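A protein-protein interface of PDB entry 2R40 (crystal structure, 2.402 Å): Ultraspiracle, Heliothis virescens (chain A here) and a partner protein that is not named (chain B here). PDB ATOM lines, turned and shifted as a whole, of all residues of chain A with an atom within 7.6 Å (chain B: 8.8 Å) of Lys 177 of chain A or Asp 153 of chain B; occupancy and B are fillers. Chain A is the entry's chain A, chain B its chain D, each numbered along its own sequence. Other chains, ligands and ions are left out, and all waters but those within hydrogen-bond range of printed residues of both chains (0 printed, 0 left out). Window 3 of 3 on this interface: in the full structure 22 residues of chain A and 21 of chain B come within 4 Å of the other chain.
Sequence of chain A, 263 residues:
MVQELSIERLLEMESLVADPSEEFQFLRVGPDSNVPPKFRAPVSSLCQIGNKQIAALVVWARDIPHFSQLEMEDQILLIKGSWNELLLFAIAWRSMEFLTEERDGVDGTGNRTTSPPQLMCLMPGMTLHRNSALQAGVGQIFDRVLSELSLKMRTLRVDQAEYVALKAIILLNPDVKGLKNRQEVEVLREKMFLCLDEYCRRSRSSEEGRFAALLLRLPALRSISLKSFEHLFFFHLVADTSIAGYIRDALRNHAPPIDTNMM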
ATOM      1  N   ASP A  74      -5.708  17.484  20.954  1.00  0.00           N
ATOM      2  CA  ASP A  74      -5.811  16.314  21.835  1.00  0.00           C
ATOM      3  C   ASP A  74      -6.470  16.675  23.160  1.00  0.00           C
ATOM      4  O   ASP A  74      -7.318  15.931  23.659  1.00  0.00           O
ATOM      5  CB  ASP A  74      -4.431  15.681  22.087  1.00  0.00           C
ATOM      6  CG  ASP A  74      -3.870  14.956  20.861  1.00  0.00           C
ATOM      7  OD1 ASP A  74      -4.543  14.914  19.808  1.00  0.00           O
ATOM      8  OD2 ASP A  74      -2.741  14.421  20.957  1.00  0.00           O
ATOM      9  N   LEU A  77     -10.105  16.825  22.706  1.00  0.00           N
ATOM     10  CA  LEU A  77     -10.637  15.476  22.544  1.00  0.00           C
ATOM     11  C   LEU A  77     -10.779  14.754  23.886  1.00  0.00           C
ATOM     12  O   LEU A  77     -11.810  14.141  24.156  1.00  0.00           O
ATOM     13  CB  LEU A  77      -9.775  14.676  21.560  1.00  0.00           C
ATOM     14  CG  LEU A  77     -10.170  14.568  20.078  1.00  0.00           C
ATOM     15  CD1 LEU A  77     -11.018  15.728  19.551  1.00  0.00           C
ATOM     16  CD2 LEU A  77      -8.949  14.370  19.206  1.00  0.00           C
ATOM     17  N   LEU A  78      -9.766  14.858  24.738  1.00  0.00           N
ATOM     18  CA  LEU A  78      -9.826  14.256  26.079  1.00  0.00           C
ATOM     19  C   LEU A  78     -10.953  14.812  26.958  1.00  0.00           C
ATOM     20  O   LEU A  78     -11.589  14.053  27.682  1.00  0.00           O
ATOM     21  CB  LEU A  78      -8.475  14.348  26.805  1.00  0.00           C
ATOM     22  CG  LEU A  78      -7.273  13.689  26.113  1.00  0.00           C
ATOM     23  CD1 LEU A  78      -5.974  14.041  26.849  1.00  0.00           C
ATOM     24  CD2 LEU A  78      -7.433  12.175  25.951  1.00  0.00           C
ATOM     25  N   ASN A 173      -7.265   9.360  28.780  1.00  0.00           N
ATOM     26  CA  ASN A 173      -7.644   8.168  28.043  1.00  0.00           C
ATOM     27  C   ASN A 173      -6.975   8.128  26.664  1.00  0.00           C
ATOM     28  O   ASN A 173      -7.361   8.875  25.768  1.00  0.00           O
ATOM     29  CB  ASN A 173      -9.178   8.099  27.930  1.00  0.00           C
ATOM     30  CG  ASN A 173      -9.672   6.868  27.169  1.00  0.00           C
ATOM     31  OD1 ASN A 173      -8.888   6.003  26.751  1.00  0.00           O
ATOM     32  ND2 ASN A 173     -10.984   6.799  26.974  1.00  0.00           N
ATOM     33  N   PRO A 174      -5.991   7.231  26.479  1.00  0.00           N
ATOM     34  CA  PRO A 174      -5.250   7.243  25.210  1.00  0.00           C
ATOM     35  C   PRO A 174      -6.007   6.579  24.050  1.00  0.00           C
ATOM     36  O   PRO A 174      -5.544   6.626  22.900  1.00  0.00           O
ATOM     37  CB  PRO A 174      -3.959   6.479  25.539  1.00  0.00           C
ATOM     38  CG  PRO A 174      -4.264   5.666  26.765  1.00  0.00           C
ATOM     39  CD  PRO A 174      -5.547   6.156  27.387  1.00  0.00           C
ATOM     40  N   ASP A 175      -7.164   5.987  24.348  1.00  0.00           N
ATOM     41  CA  ASP A 175      -7.959   5.271  23.352  1.00  0.00           C
ATOM     42  C   ASP A 175      -9.035   6.166  22.714  1.00  0.00           C
ATOM     43  O   ASP A 175      -9.881   5.684  21.945  1.00  0.00           O
ATOM     44  CB  ASP A 175      -8.593   4.030  23.985  1.00  0.00           C
ATOM     45  CG  ASP A 175      -7.565   2.957  24.361  1.00  0.00           C
ATOM     46  OD1 ASP A 175      -6.481   2.855  23.734  1.00  0.00           O
ATOM     47  OD2 ASP A 175      -7.854   2.204  25.312  1.00  0.00           O
ATOM     48  N   VAL A 176      -8.990   7.462  23.041  1.00  0.00           N
ATOM     49  CA  VAL A 176      -9.878   8.460  22.457  1.00  0.00           C
ATOM     50  C   VAL A 176      -9.602   8.587  20.967  1.00  0.00           C
ATOM     51  O   VAL A 176      -8.457   8.733  20.535  1.00  0.00           O
ATOM     52  CB  VAL A 176      -9.808   9.841  23.199  1.00  0.00           C
ATOM     53  CG1 VAL A 176     -10.386  10.967  22.353  1.00  0.00           C
ATOM     54  CG2 VAL A 176     -10.580   9.776  24.524  1.00  0.00           C
ATOM     55  N   LYS A 177     -10.673   8.510  20.187  1.00  0.00           N
ATOM     56  CA  LYS A 177     -10.568   8.490  18.736  1.00  0.00           C
ATOM     57  C   LYS A 177     -10.122   9.841  18.167  1.00  0.00           C
ATOM     58  O   LYS A 177     -10.739  10.874  18.429  1.00  0.00           O
ATOM     59  CB  LYS A 177     -11.901   8.032  18.127  1.00  0.00           C
ATOM     60  CG  LYS A 177     -11.740   7.159  16.886  1.00  0.00           C
ATOM     61  CD  LYS A 177     -13.018   6.383  16.507  1.00  0.00           C
ATOM     62  CE  LYS A 177     -14.175   7.298  16.086  1.00  0.00           C
ATOM     63  NZ  LYS A 177     -14.915   7.846  17.269  1.00  0.00           N
ATOM     64  N   GLY A 178      -9.029   9.822  17.408  1.00  0.00           N
ATOM     65  CA  GLY A 178      -8.533  11.016  16.722  1.00  0.00           C
ATOM     66  C   GLY A 178      -7.363  11.744  17.370  1.00  0.00           C
ATOM     67  O   GLY A 178      -6.941  12.805  16.882  1.00  0.00           O
ATOM     68  N   LEU A 179      -6.850  11.193  18.470  1.00  0.00           N
ATOM     69  CA  LEU A 179      -5.665  11.730  19.138  1.00  0.00           C
ATOM     70  C   LEU A 179      -4.453  11.764  18.212  1.00  0.00           C
ATOM     71  O   LEU A 179      -4.220  10.823  17.444  1.00  0.00           O
ATOM     72  CB  LEU A 179      -5.307  10.882  20.358  1.00  0.00           C
ATOM     73  CG  LEU A 179      -6.167  10.954  21.610  1.00  0.00           C
ATOM     74  CD1 LEU A 179      -5.671   9.910  22.588  1.00  0.00           C
ATOM     75  CD2 LEU A 179      -6.161  12.354  22.242  1.00  0.00           C
ATOM     76  N   LYS A 180      -3.680  12.844  18.297  1.00  0.00           N
ATOM     77  CA  LYS A 180      -2.434  12.945  17.544  1.00  0.00           C
ATOM     78  C   LYS A 180      -1.319  12.181  18.247  1.00  0.00           C
ATOM     79  O   LYS A 180      -0.852  11.165  17.732  1.00  0.00           O
ATOM     80  CB  LYS A 180      -2.025  14.405  17.322  1.00  0.00           C
ATOM     81  CG  LYS A 180      -2.834  15.131  16.274  1.00  0.00           C
ATOM     82  CD  LYS A 180      -2.543  16.620  16.322  1.00  0.00           C
ATOM     83  CE  LYS A 180      -3.771  17.434  15.939  1.00  0.00           C
ATOM     84  NZ  LYS A 180      -3.511  18.907  15.879  1.00  0.00           N
ATOM     85  N   ARG A 182      -0.937  10.014  20.779  1.00  0.00           N
ATOM     86  CA  ARG A 182      -1.516   8.965  21.611  1.00  0.00           C
ATOM     87  C   ARG A 182      -0.604   8.521  22.771  1.00  0.00           C
ATOM     88  O   ARG A 182      -1.061   8.367  23.909  1.00  0.00           O
ATOM     89  CB  ARG A 182      -1.855   7.778  20.708  1.00  0.00           C
ATOM     90  CG  ARG A 182      -2.730   6.743  21.343  1.00  0.00           C
ATOM     91  CD  ARG A 182      -2.461   5.348  20.785  1.00  0.00           C
ATOM     92  NE  ARG A 182      -2.643   4.351  21.841  1.00  0.00           N
ATOM     93  CZ  ARG A 182      -3.820   3.854  22.217  1.00  0.00           C
ATOM     94  NH1 ARG A 182      -4.941   4.235  21.618  1.00  0.00           N
ATOM     95  NH2 ARG A 182      -3.875   2.966  23.198  1.00  0.00           N
ATOM     96  N   MET B 115     -16.372  -8.821  21.538  1.00  0.00           N
ATOM     97  CA  MET B 115     -15.399  -7.798  21.147  1.00  0.00           C
ATOM     98  C   MET B 115     -13.954  -8.248  21.345  1.00  0.00           C
ATOM     99  O   MET B 115     -13.061  -7.819  20.612  1.00  0.00           O
ATOM    100  CB  MET B 115     -15.646  -6.488  21.914  1.00  0.00           C
ATOM    101  CG  MET B 115     -17.008  -5.894  21.720  1.00  0.00           C
ATOM    102  SD  MET B 115     -17.504  -5.755  19.993  1.00  0.00           S
ATOM    103  CE  MET B 115     -19.282  -5.757  20.181  1.00  0.00           C
ATOM    104  N   VAL B 118     -13.154 -10.738  18.389  1.00  0.00           N
ATOM    105  CA  VAL B 118     -12.816 -10.114  17.102  1.00  0.00           C
ATOM    106  C   VAL B 118     -11.402  -9.504  17.146  1.00  0.00           C
ATOM    107  O   VAL B 118     -10.667  -9.555  16.154  1.00  0.00           O
ATOM    108  CB  VAL B 118     -13.894  -9.076  16.624  1.00  0.00           C
ATOM    109  CG1 VAL B 118     -14.284  -8.168  17.721  1.00  0.00           C
ATOM    110  CG2 VAL B 118     -13.398  -8.231  15.463  1.00  0.00           C
ATOM    111  N   ARG B 139     -14.036  -2.871   6.331  1.00  0.00           N
ATOM    112  CA  ARG B 139     -14.999  -1.787   6.506  1.00  0.00           C
ATOM    113  C   ARG B 139     -16.100  -1.817   5.418  1.00  0.00           C
ATOM    114  O   ARG B 139     -17.284  -1.589   5.703  1.00  0.00           O
ATOM    115  CB  ARG B 139     -14.241  -0.463   6.477  1.00  0.00           C
ATOM    116  CG  ARG B 139     -14.794   0.633   7.353  1.00  0.00           C
ATOM    117  CD  ARG B 139     -13.830   1.813   7.391  1.00  0.00           C
ATOM    118  NE  ARG B 139     -12.894   1.742   8.523  1.00  0.00           N
ATOM    119  CZ  ARG B 139     -11.642   1.290   8.454  1.00  0.00           C
ATOM    120  NH1 ARG B 139     -11.143   0.850   7.304  1.00  0.00           N
ATOM    121  NH2 ARG B 139     -10.889   1.275   9.547  1.00  0.00           N
ATOM    122  N   MET B 147     -24.026  -2.326   8.189  1.00  0.00           N
ATOM    123  CA  MET B 147     -23.488  -2.215   9.551  1.00  0.00           C
ATOM    124  C   MET B 147     -22.267  -1.309   9.651  1.00  0.00           C
ATOM    125  O   MET B 147     -21.372  -1.536  10.471  1.00  0.00           O
ATOM    126  CB  MET B 147     -23.210  -3.610  10.118  1.00  0.00           C
ATOM    127  CG  MET B 147     -24.450  -4.476  10.107  1.00  0.00           C
ATOM    128  SD  MET B 147     -24.189  -6.022  10.934  1.00  0.00           S
ATOM    129  CE  MET B 147     -25.537  -7.002  10.278  1.00  0.00           C
ATOM    130  N   ALA B 148     -22.263  -0.271   8.824  1.00  0.00           N
ATOM    131  CA  ALA B 148     -21.252   0.784   8.829  1.00  0.00           C
ATOM    132  C   ALA B 148     -21.175   1.539  10.157  1.00  0.00           C
ATOM    133  O   ALA B 148     -20.134   2.098  10.491  1.00  0.00           O
ATOM    134  CB  ALA B 148     -21.524   1.767   7.686  1.00  0.00           C
ATOM    135  N   TYR B 149     -22.278   1.552  10.899  1.00  0.00           N
ATOM    136  CA  TYR B 149     -22.365   2.256  12.172  1.00  0.00           C
ATOM    137  C   TYR B 149     -21.383   1.662  13.172  1.00  0.00           C
ATOM    138  O   TYR B 149     -20.787   2.359  13.981  1.00  0.00           O
ATOM    139  CB  TYR B 149     -23.806   2.200  12.713  1.00  0.00           C
ATOM    140  CG  TYR B 149     -23.944   2.574  14.173  1.00  0.00           C
ATOM    141  CD1 TYR B 149     -23.939   3.912  14.581  1.00  0.00           C
ATOM    142  CD2 TYR B 149     -24.070   1.585  15.153  1.00  0.00           C
ATOM    143  CE1 TYR B 149     -24.046   4.248  15.935  1.00  0.00           C
ATOM    144  CE2 TYR B 149     -24.178   1.905  16.489  1.00  0.00           C
ATOM    145  CZ  TYR B 149     -24.167   3.233  16.876  1.00  0.00           C
ATOM    146  OH  TYR B 149     -24.269   3.537  18.210  1.00  0.00           O
ATOM    147  N   VAL B 150     -21.203   0.359  13.079  1.00  0.00           N
ATOM    148  CA  VAL B 150     -20.532  -0.402  14.104  1.00  0.00           C
ATOM    149  C   VAL B 150     -19.017  -0.612  13.849  1.00  0.00           C
ATOM    150  O   VAL B 150     -18.226  -0.722  14.794  1.00  0.00           O
ATOM    151  CB  VAL B 150     -21.337  -1.717  14.348  1.00  0.00           C
ATOM    152  CG1 VAL B 150     -20.534  -2.974  14.042  1.00  0.00           C
ATOM    153  CG2 VAL B 150     -21.956  -1.726  15.753  1.00  0.00           C
ATOM    154  N   ILE B 151     -18.611  -0.591  12.584  1.00  0.00           N
ATOM    155  CA  ILE B 151     -17.296  -1.105  12.217  1.00  0.00           C
ATOM    156  C   ILE B 151     -16.117  -0.163  12.533  1.00  0.00           C
ATOM    157  O   ILE B 151     -15.015  -0.618  12.821  1.00  0.00           O
ATOM    158  CB  ILE B 151     -17.279  -1.676  10.740  1.00  0.00           C
ATOM    159  CG1 ILE B 151     -15.969  -2.418  10.440  1.00  0.00           C
ATOM    160  CG2 ILE B 151     -17.603  -0.598   9.702  1.00  0.00           C
ATOM    161  CD1 ILE B 151     -15.800  -3.695  11.249  1.00  0.00           C
ATOM    162  N   GLU B 152     -16.363   1.140  12.516  1.00  0.00           N
ATOM    163  CA  GLU B 152     -15.321   2.120  12.787  1.00  0.00           C
ATOM    164  C   GLU B 152     -14.695   1.936  14.175  1.00  0.00           C
ATOM    165  O   GLU B 152     -13.483   1.798  14.306  1.00  0.00           O
ATOM    166  CB  GLU B 152     -15.899   3.532  12.689  1.00  0.00           C
ATOM    167  CG  GLU B 152     -14.923   4.577  12.212  1.00  0.00           C
ATOM    168  CD  GLU B 152     -14.848   4.617  10.707  1.00  0.00           C
ATOM    169  OE1 GLU B 152     -14.238   3.691  10.112  1.00  0.00           O
ATOM    170  OE2 GLU B 152     -15.400   5.574  10.118  1.00  0.00           O
ATOM    171  N   ASP B 153     -15.542   1.959  15.197  1.00  0.00           N
ATOM    172  CA  ASP B 153     -15.108   1.906  16.578  1.00  0.00           C
ATOM    173  C   ASP B 153     -14.611   0.519  16.939  1.00  0.00           C
ATOM    174  O   ASP B 153     -13.749   0.369  17.807  1.00  0.00           O
ATOM    175  CB  ASP B 153     -16.240   2.340  17.505  1.00  0.00           C
ATOM    176  CG  ASP B 153     -16.592   3.816  17.350  1.00  0.00           C
ATOM    177  OD1 ASP B 153     -15.722   4.631  16.975  1.00  0.00           O
ATOM    178  OD2 ASP B 153     -17.756   4.168  17.611  1.00  0.00           O
ATOM    179  N   LEU B 154     -15.142  -0.481  16.242  1.00  0.00           N
ATOM    180  CA  LEU B 154     -14.694  -1.841  16.401  1.00  0.00           C
ATOM    181  C   LEU B 154     -13.248  -2.040  15.921  1.00  0.00           C
ATOM    182  O   LEU B 154     -12.456  -2.651  16.617  1.00  0.00           O
ATOM    183  CB  LEU B 154     -15.647  -2.799  15.686  1.00  0.00           C
ATOM    184  CG  LEU B 154     -15.429  -4.308  15.811  1.00  0.00           C
ATOM    185  CD1 LEU B 154     -15.235  -4.726  17.271  1.00  0.00           C
ATOM    186  CD2 LEU B 154     -16.633  -5.032  15.186  1.00  0.00           C
ATOM    187  N   LEU B 155     -12.917  -1.521  14.742  1.00  0.00           N
ATOM    188  CA  LEU B 155     -11.591  -1.669  14.178  1.00  0.00           C
ATOM    189  C   LEU B 155     -10.558  -0.853  14.964  1.00  0.00           C
ATOM    190  O   LEU B 155      -9.402  -1.286  15.146  1.00  0.00           O
ATOM    191  CB  LEU B 155     -11.610  -1.276  12.704  1.00  0.00           C
ATOM    192  CG  LEU B 155     -11.630  -2.369  11.608  1.00  0.00           C
ATOM    193  CD1 LEU B 155     -12.122  -3.752  12.056  1.00  0.00           C
ATOM    194  CD2 LEU B 155     -12.337  -1.884  10.342  1.00  0.00           C
ATOM    195  N   HIS B 156     -10.987   0.315  15.444  1.00  0.00           N
ATOM    196  CA  HIS B 156     -10.168   1.149  16.313  1.00  0.00           C
ATOM    197  C   HIS B 156      -9.830   0.395  17.594  1.00  0.00           C
ATOM    198  O   HIS B 156      -8.674   0.386  18.020  1.00  0.00           O
ATOM    199  CB  HIS B 156     -10.883   2.471  16.619  1.00  0.00           C
ATOM    200  CG  HIS B 156     -10.245   3.257  17.720  1.00  0.00           C
ATOM    201  ND1 HIS B 156      -9.102   4.008  17.536  1.00  0.00           N
ATOM    202  CD2 HIS B 156     -10.590   3.405  19.023  1.00  0.00           C
ATOM    203  CE1 HIS B 156      -8.772   4.588  18.676  1.00  0.00           C
ATOM    204  NE2 HIS B 156      -9.658   4.241  19.594  1.00  0.00           N
ATOM    205  N   PHE B 157     -10.833  -0.245  18.190  1.00  0.00           N
ATOM    206  CA  PHE B 157     -10.651  -1.068  19.376  1.00  0.00           C
ATOM    207  C   PHE B 157      -9.640  -2.180  19.099  1.00  0.00           C
ATOM    208  O   PHE B 157      -8.705  -2.378  19.885  1.00  0.00           O
ATOM    209  CB  PHE B 157     -11.986  -1.674  19.829  1.00  0.00           C
ATOM    210  CG  PHE B 157     -11.847  -2.705  20.927  1.00  0.00           C
ATOM    211  CD1 PHE B 157     -11.669  -2.313  22.249  1.00  0.00           C
ATOM    212  CD2 PHE B 157     -11.912  -4.051  20.641  1.00  0.00           C
ATOM    213  CE1 PHE B 157     -11.526  -3.265  23.267  1.00  0.00           C
ATOM    214  CE2 PHE B 157     -11.773  -5.012  21.641  1.00  0.00           C
ATOM    215  CZ  PHE B 157     -11.568  -4.621  22.960  1.00  0.00           C
ATOM    216  N   CYS B 158      -9.850  -2.892  17.987  1.00  0.00           N
ATOM    217  CA  CYS B 158      -8.913  -3.902  17.484  1.00  0.00           C
ATOM    218  C   CYS B 158      -7.468  -3.423  17.344  1.00  0.00           C
ATOM    219  O   CYS B 158      -6.567  -4.101  17.816  1.00  0.00           O
ATOM    220  CB  CYS B 158      -9.401  -4.464  16.144  1.00  0.00           C
ATOM    221  SG  CYS B 158     -10.860  -5.496  16.332  1.00  0.00           S
ATOM    222  N   ARG B 159      -7.253  -2.271  16.701  1.00  0.00           N
ATOM    223  CA  ARG B 159      -5.926  -1.636  16.639  1.00  0.00           C
ATOM    224  C   ARG B 159      -5.334  -1.381  18.030  1.00  0.00           C
ATOM    225  O   ARG B 159      -4.194  -1.714  18.269  1.00  0.00           O
ATOM    226  CB  ARG B 159      -5.967  -0.309  15.868  1.00  0.00           C
ATOM    227  CG  ARG B 159      -6.168  -0.439  14.373  1.00  0.00           C
ATOM    228  CD  ARG B 159      -6.016   0.929  13.657  1.00  0.00           C
ATOM    229  NE  ARG B 159      -7.236   1.740  13.685  1.00  0.00           N
ATOM    230  CZ  ARG B 159      -8.334   1.494  12.967  1.00  0.00           C
ATOM    231  NH1 ARG B 159      -8.380   0.449  12.149  1.00  0.00           N
ATOM    232  NH2 ARG B 159      -9.394   2.297  13.071  1.00  0.00           N
ATOM    233  N   CYS B 160      -6.112  -0.776  18.928  1.00  0.00           N
ATOM    234  CA  CYS B 160      -5.675  -0.503  20.308  1.00  0.00           C
ATOM    235  C   CYS B 160      -5.426  -1.789  21.098  1.00  0.00           C
ATOM    236  O   CYS B 160      -4.575  -1.819  21.974  1.00  0.00           O
ATOM    237  CB  CYS B 160      -6.711   0.339  21.049  1.00  0.00           C
ATOM    238  SG  CYS B 160      -6.922   2.003  20.405  1.00  0.00           S
ATOM    239  N   MET B 161      -6.191  -2.827  20.770  1.00  0.00           N
ATOM    240  CA  MET B 161      -6.158  -4.140  21.420  1.00  0.00           C
ATOM    241  C   MET B 161      -5.078  -5.059  20.941  1.00  0.00           C
ATOM    242  O   MET B 161      -4.660  -5.929  21.679  1.00  0.00           O
ATOM    243  CB  MET B 161      -7.470  -4.890  21.177  1.00  0.00           C
ATOM    244  CG  MET B 161      -8.501  -4.643  22.197  1.00  0.00           C
ATOM    245  SD  MET B 161      -7.744  -4.484  23.790  1.00  0.00           S
ATOM    246  CE  MET B 161      -7.694  -2.671  24.008  1.00  0.00           C
ATOM    247  N   GLU B 230     -13.849   0.093  27.771  1.00  0.00           N
ATOM    248  CA  GLU B 230     -14.028   0.314  26.331  1.00  0.00           C
ATOM    249  C   GLU B 230     -14.980  -0.693  25.669  1.00  0.00           C
ATOM    250  O   GLU B 230     -15.669  -0.358  24.710  1.00  0.00           O
ATOM    251  CB  GLU B 230     -12.675   0.362  25.596  1.00  0.00           C
ATOM    252  CG  GLU B 230     -11.700   1.463  26.083  1.00  0.00           C
ATOM    253  CD  GLU B 230     -12.305   2.861  26.132  1.00  0.00           C
ATOM    254  OE1 GLU B 230     -12.995   3.261  25.163  1.00  0.00           O
ATOM    255  OE2 GLU B 230     -12.086   3.579  27.146  1.00  0.00           O
ATOM    256  N   ILE B 231     -15.046  -1.913  26.179  1.00  0.00           N
ATOM    257  CA  ILE B 231     -16.039  -2.856  25.662  1.00  0.00           C
ATOM    258  C   ILE B 231     -17.498  -2.580  26.100  1.00  0.00           C
ATOM    259  O   ILE B 231     -18.429  -3.143  25.504  1.00  0.00           O
ATOM    260  CB  ILE B 231     -15.652  -4.319  25.922  1.00  0.00           C
ATOM    261  CG1 ILE B 231     -15.612  -4.641  27.418  1.00  0.00           C
ATOM    262  CG2 ILE B 231     -14.327  -4.683  25.194  1.00  0.00           C
ATOM    263  CD1 ILE B 231     -15.259  -6.081  27.706  1.00  0.00           C
ATOM    264  N   THR B 233     -18.861   0.512  25.849  1.00  0.00           N
ATOM    265  CA  THR B 233     -19.220   1.300  24.673  1.00  0.00           C
ATOM    266  C   THR B 233     -19.554   0.441  23.451  1.00  0.00           C
ATOM    267  O   THR B 233     -20.608   0.639  22.838  1.00  0.00           O
ATOM    268  CB  THR B 233     -18.106   2.275  24.299  1.00  0.00           C
ATOM    269  OG1 THR B 233     -17.759   3.026  25.457  1.00  0.00           O
ATOM    270  CG2 THR B 233     -18.546   3.233  23.213  1.00  0.00           C
ATOM    271  N   LEU B 234     -18.667  -0.495  23.100  1.00  0.00           N
ATOM    272  CA  LEU B 234     -18.883  -1.344  21.940  1.00  0.00           C
ATOM    273  C   LEU B 234     -20.105  -2.245  22.078  1.00  0.00           C
ATOM    274  O   LEU B 234     -20.862  -2.422  21.106  1.00  0.00           O
ATOM    275  CB  LEU B 234     -17.654  -2.182  21.628  1.00  0.00           C
ATOM    276  CG  LEU B 234     -16.365  -1.442  21.267  1.00  0.00           C
ATOM    277  CD1 LEU B 234     -15.197  -2.430  21.320  1.00  0.00           C
ATOM    278  CD2 LEU B 234     -16.433  -0.762  19.913  1.00  0.00           C
ATOM    279  N   GLY B 235     -20.295  -2.808  23.272  1.00  0.00           N
ATOM    280  CA  GLY B 235     -21.474  -3.618  23.573  1.00  0.00           C
ATOM    281  C   GLY B 235     -22.770  -2.852  23.412  1.00  0.00           C
ATOM    282  O   GLY B 235     -23.756  -3.380  22.879  1.00  0.00           O
ATOM    283  N   GLN B 237     -23.111  -0.087  21.548  1.00  0.00           N
ATOM    284  CA  GLN B 237     -23.198   0.130  20.099  1.00  0.00           C
ATOM    285  C   GLN B 237     -23.792  -1.090  19.377  1.00  0.00           C
ATOM    286  O   GLN B 237     -24.595  -0.931  18.449  1.00  0.00           O
ATOM    287  CB  GLN B 237     -21.843   0.496  19.504  1.00  0.00           C
ATOM    288  CG  GLN B 237     -21.360   1.885  19.910  1.00  0.00           C
ATOM    289  CD  GLN B 237     -20.085   2.326  19.194  1.00  0.00           C
ATOM    290  OE1 GLN B 237     -19.525   1.602  18.376  1.00  0.00           O
ATOM    291  NE2 GLN B 237     -19.623   3.525  19.514  1.00  0.00           N
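The side-chain amide nitrogen (NE2) of Gln 237 of chain B is in hydrogen-bond range of the side-chain carboxylate (OD2) of Asp 153 of chain B, at 2.7 Å.
The backbone carbonyl oxygen (O) of His 156 of chain B lies within hydrogen-bond range of the side-chain sulfur (SG) of Cys 160 of chain B (3.4 Å).
OD1 of Asn 173 of chain A lies within hydrogen-bond range of N of Asp 175 of chain A (3.0 Å).
O of Pro 174 of chain A lies within hydrogen-bond range of NH1 of Arg 182 of chain A (2.8 Å).
The side-chain carboxylate of Asp 175 of chain A lies within salt-bridge range of the guanidinium group of Arg 182 of chain A, at 2.7 Å.
Glu 230 of chain B touches Asp 175 of chain A (CG to OD2, 3.99 Å).
Along chain A the printed residues that touch a printed residue of chain B span positions 173 to 182.
Hydrophobic or aromatic side chains of chain B within 4 Å of the printed part of chain A: His 156.
Among the printed residues, Asp or Glu carboxylates within 4 Å of a Lys or Arg side-chain nitrogen of the other chain: Lys 177 of chain A with Asp 153 of chain B (3.3 Å).
OD1 of Asp 153 of chain B is in salt-bridge range of NZ of Lys 177 of chain A (3.3 Å).
NE2 of His 156 of chain B sits at hydrogen-bond distance from O of Asp 175 of chain A (2.8 Å).
OD1 of Asp 175 of chain A sits at hydrogen-bond distance from SG of Cys 160 of chain B, 3.5 Å away.
The side-chain sulfur of Cys 160 of chain B is in hydrogen-bond range of the guanidinium group of Arg 182 of chain A (3.2 Å).
The side-chain amide nitrogen of Asn 173 of chain A is in hydrogen-bond range of the side-chain carboxylate of Glu 230 of chain B (3.4 Å).
Of chain B, only Asp 153 comes within 4 Å of Lys 177 of chain A.
Of chain A, only Lys 177 (3.2 Å) comes within 4 Å of Asp 153 of chain B.
No residue of chain B comes within 4 Å of Val 176 of chain A.
Printed residues of chain A within 4 Å of Cys 160 of chain B: Asp 175 (3.5 Å) and Arg 182 (3.2 Å).
Printed residues of chain B within 4 Å of Arg 182 of chain A: Cys 160.
Of the printed residues of chain A, Glu 230 of chain B touches Asn 173 (3.4 Å) and Asp 175 (3.99 Å).
Printed residues of chain B within 4 Å of Asp 175 of chain A: His 156, Cys 160 and Glu 230.
Leu 78 of chain A touches none of the printed residues of chain B.
Leu 77 of chain A touches none of the printed residues of chain B.
The nearest residue of chain B that does not touch Lys 177 of chain A is His 156 of chain B (4.2 Å).
The nearest printed residue of chain A that does not touch Asp 153 of chain B is Asp 175 of chain A (7.7 Å).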
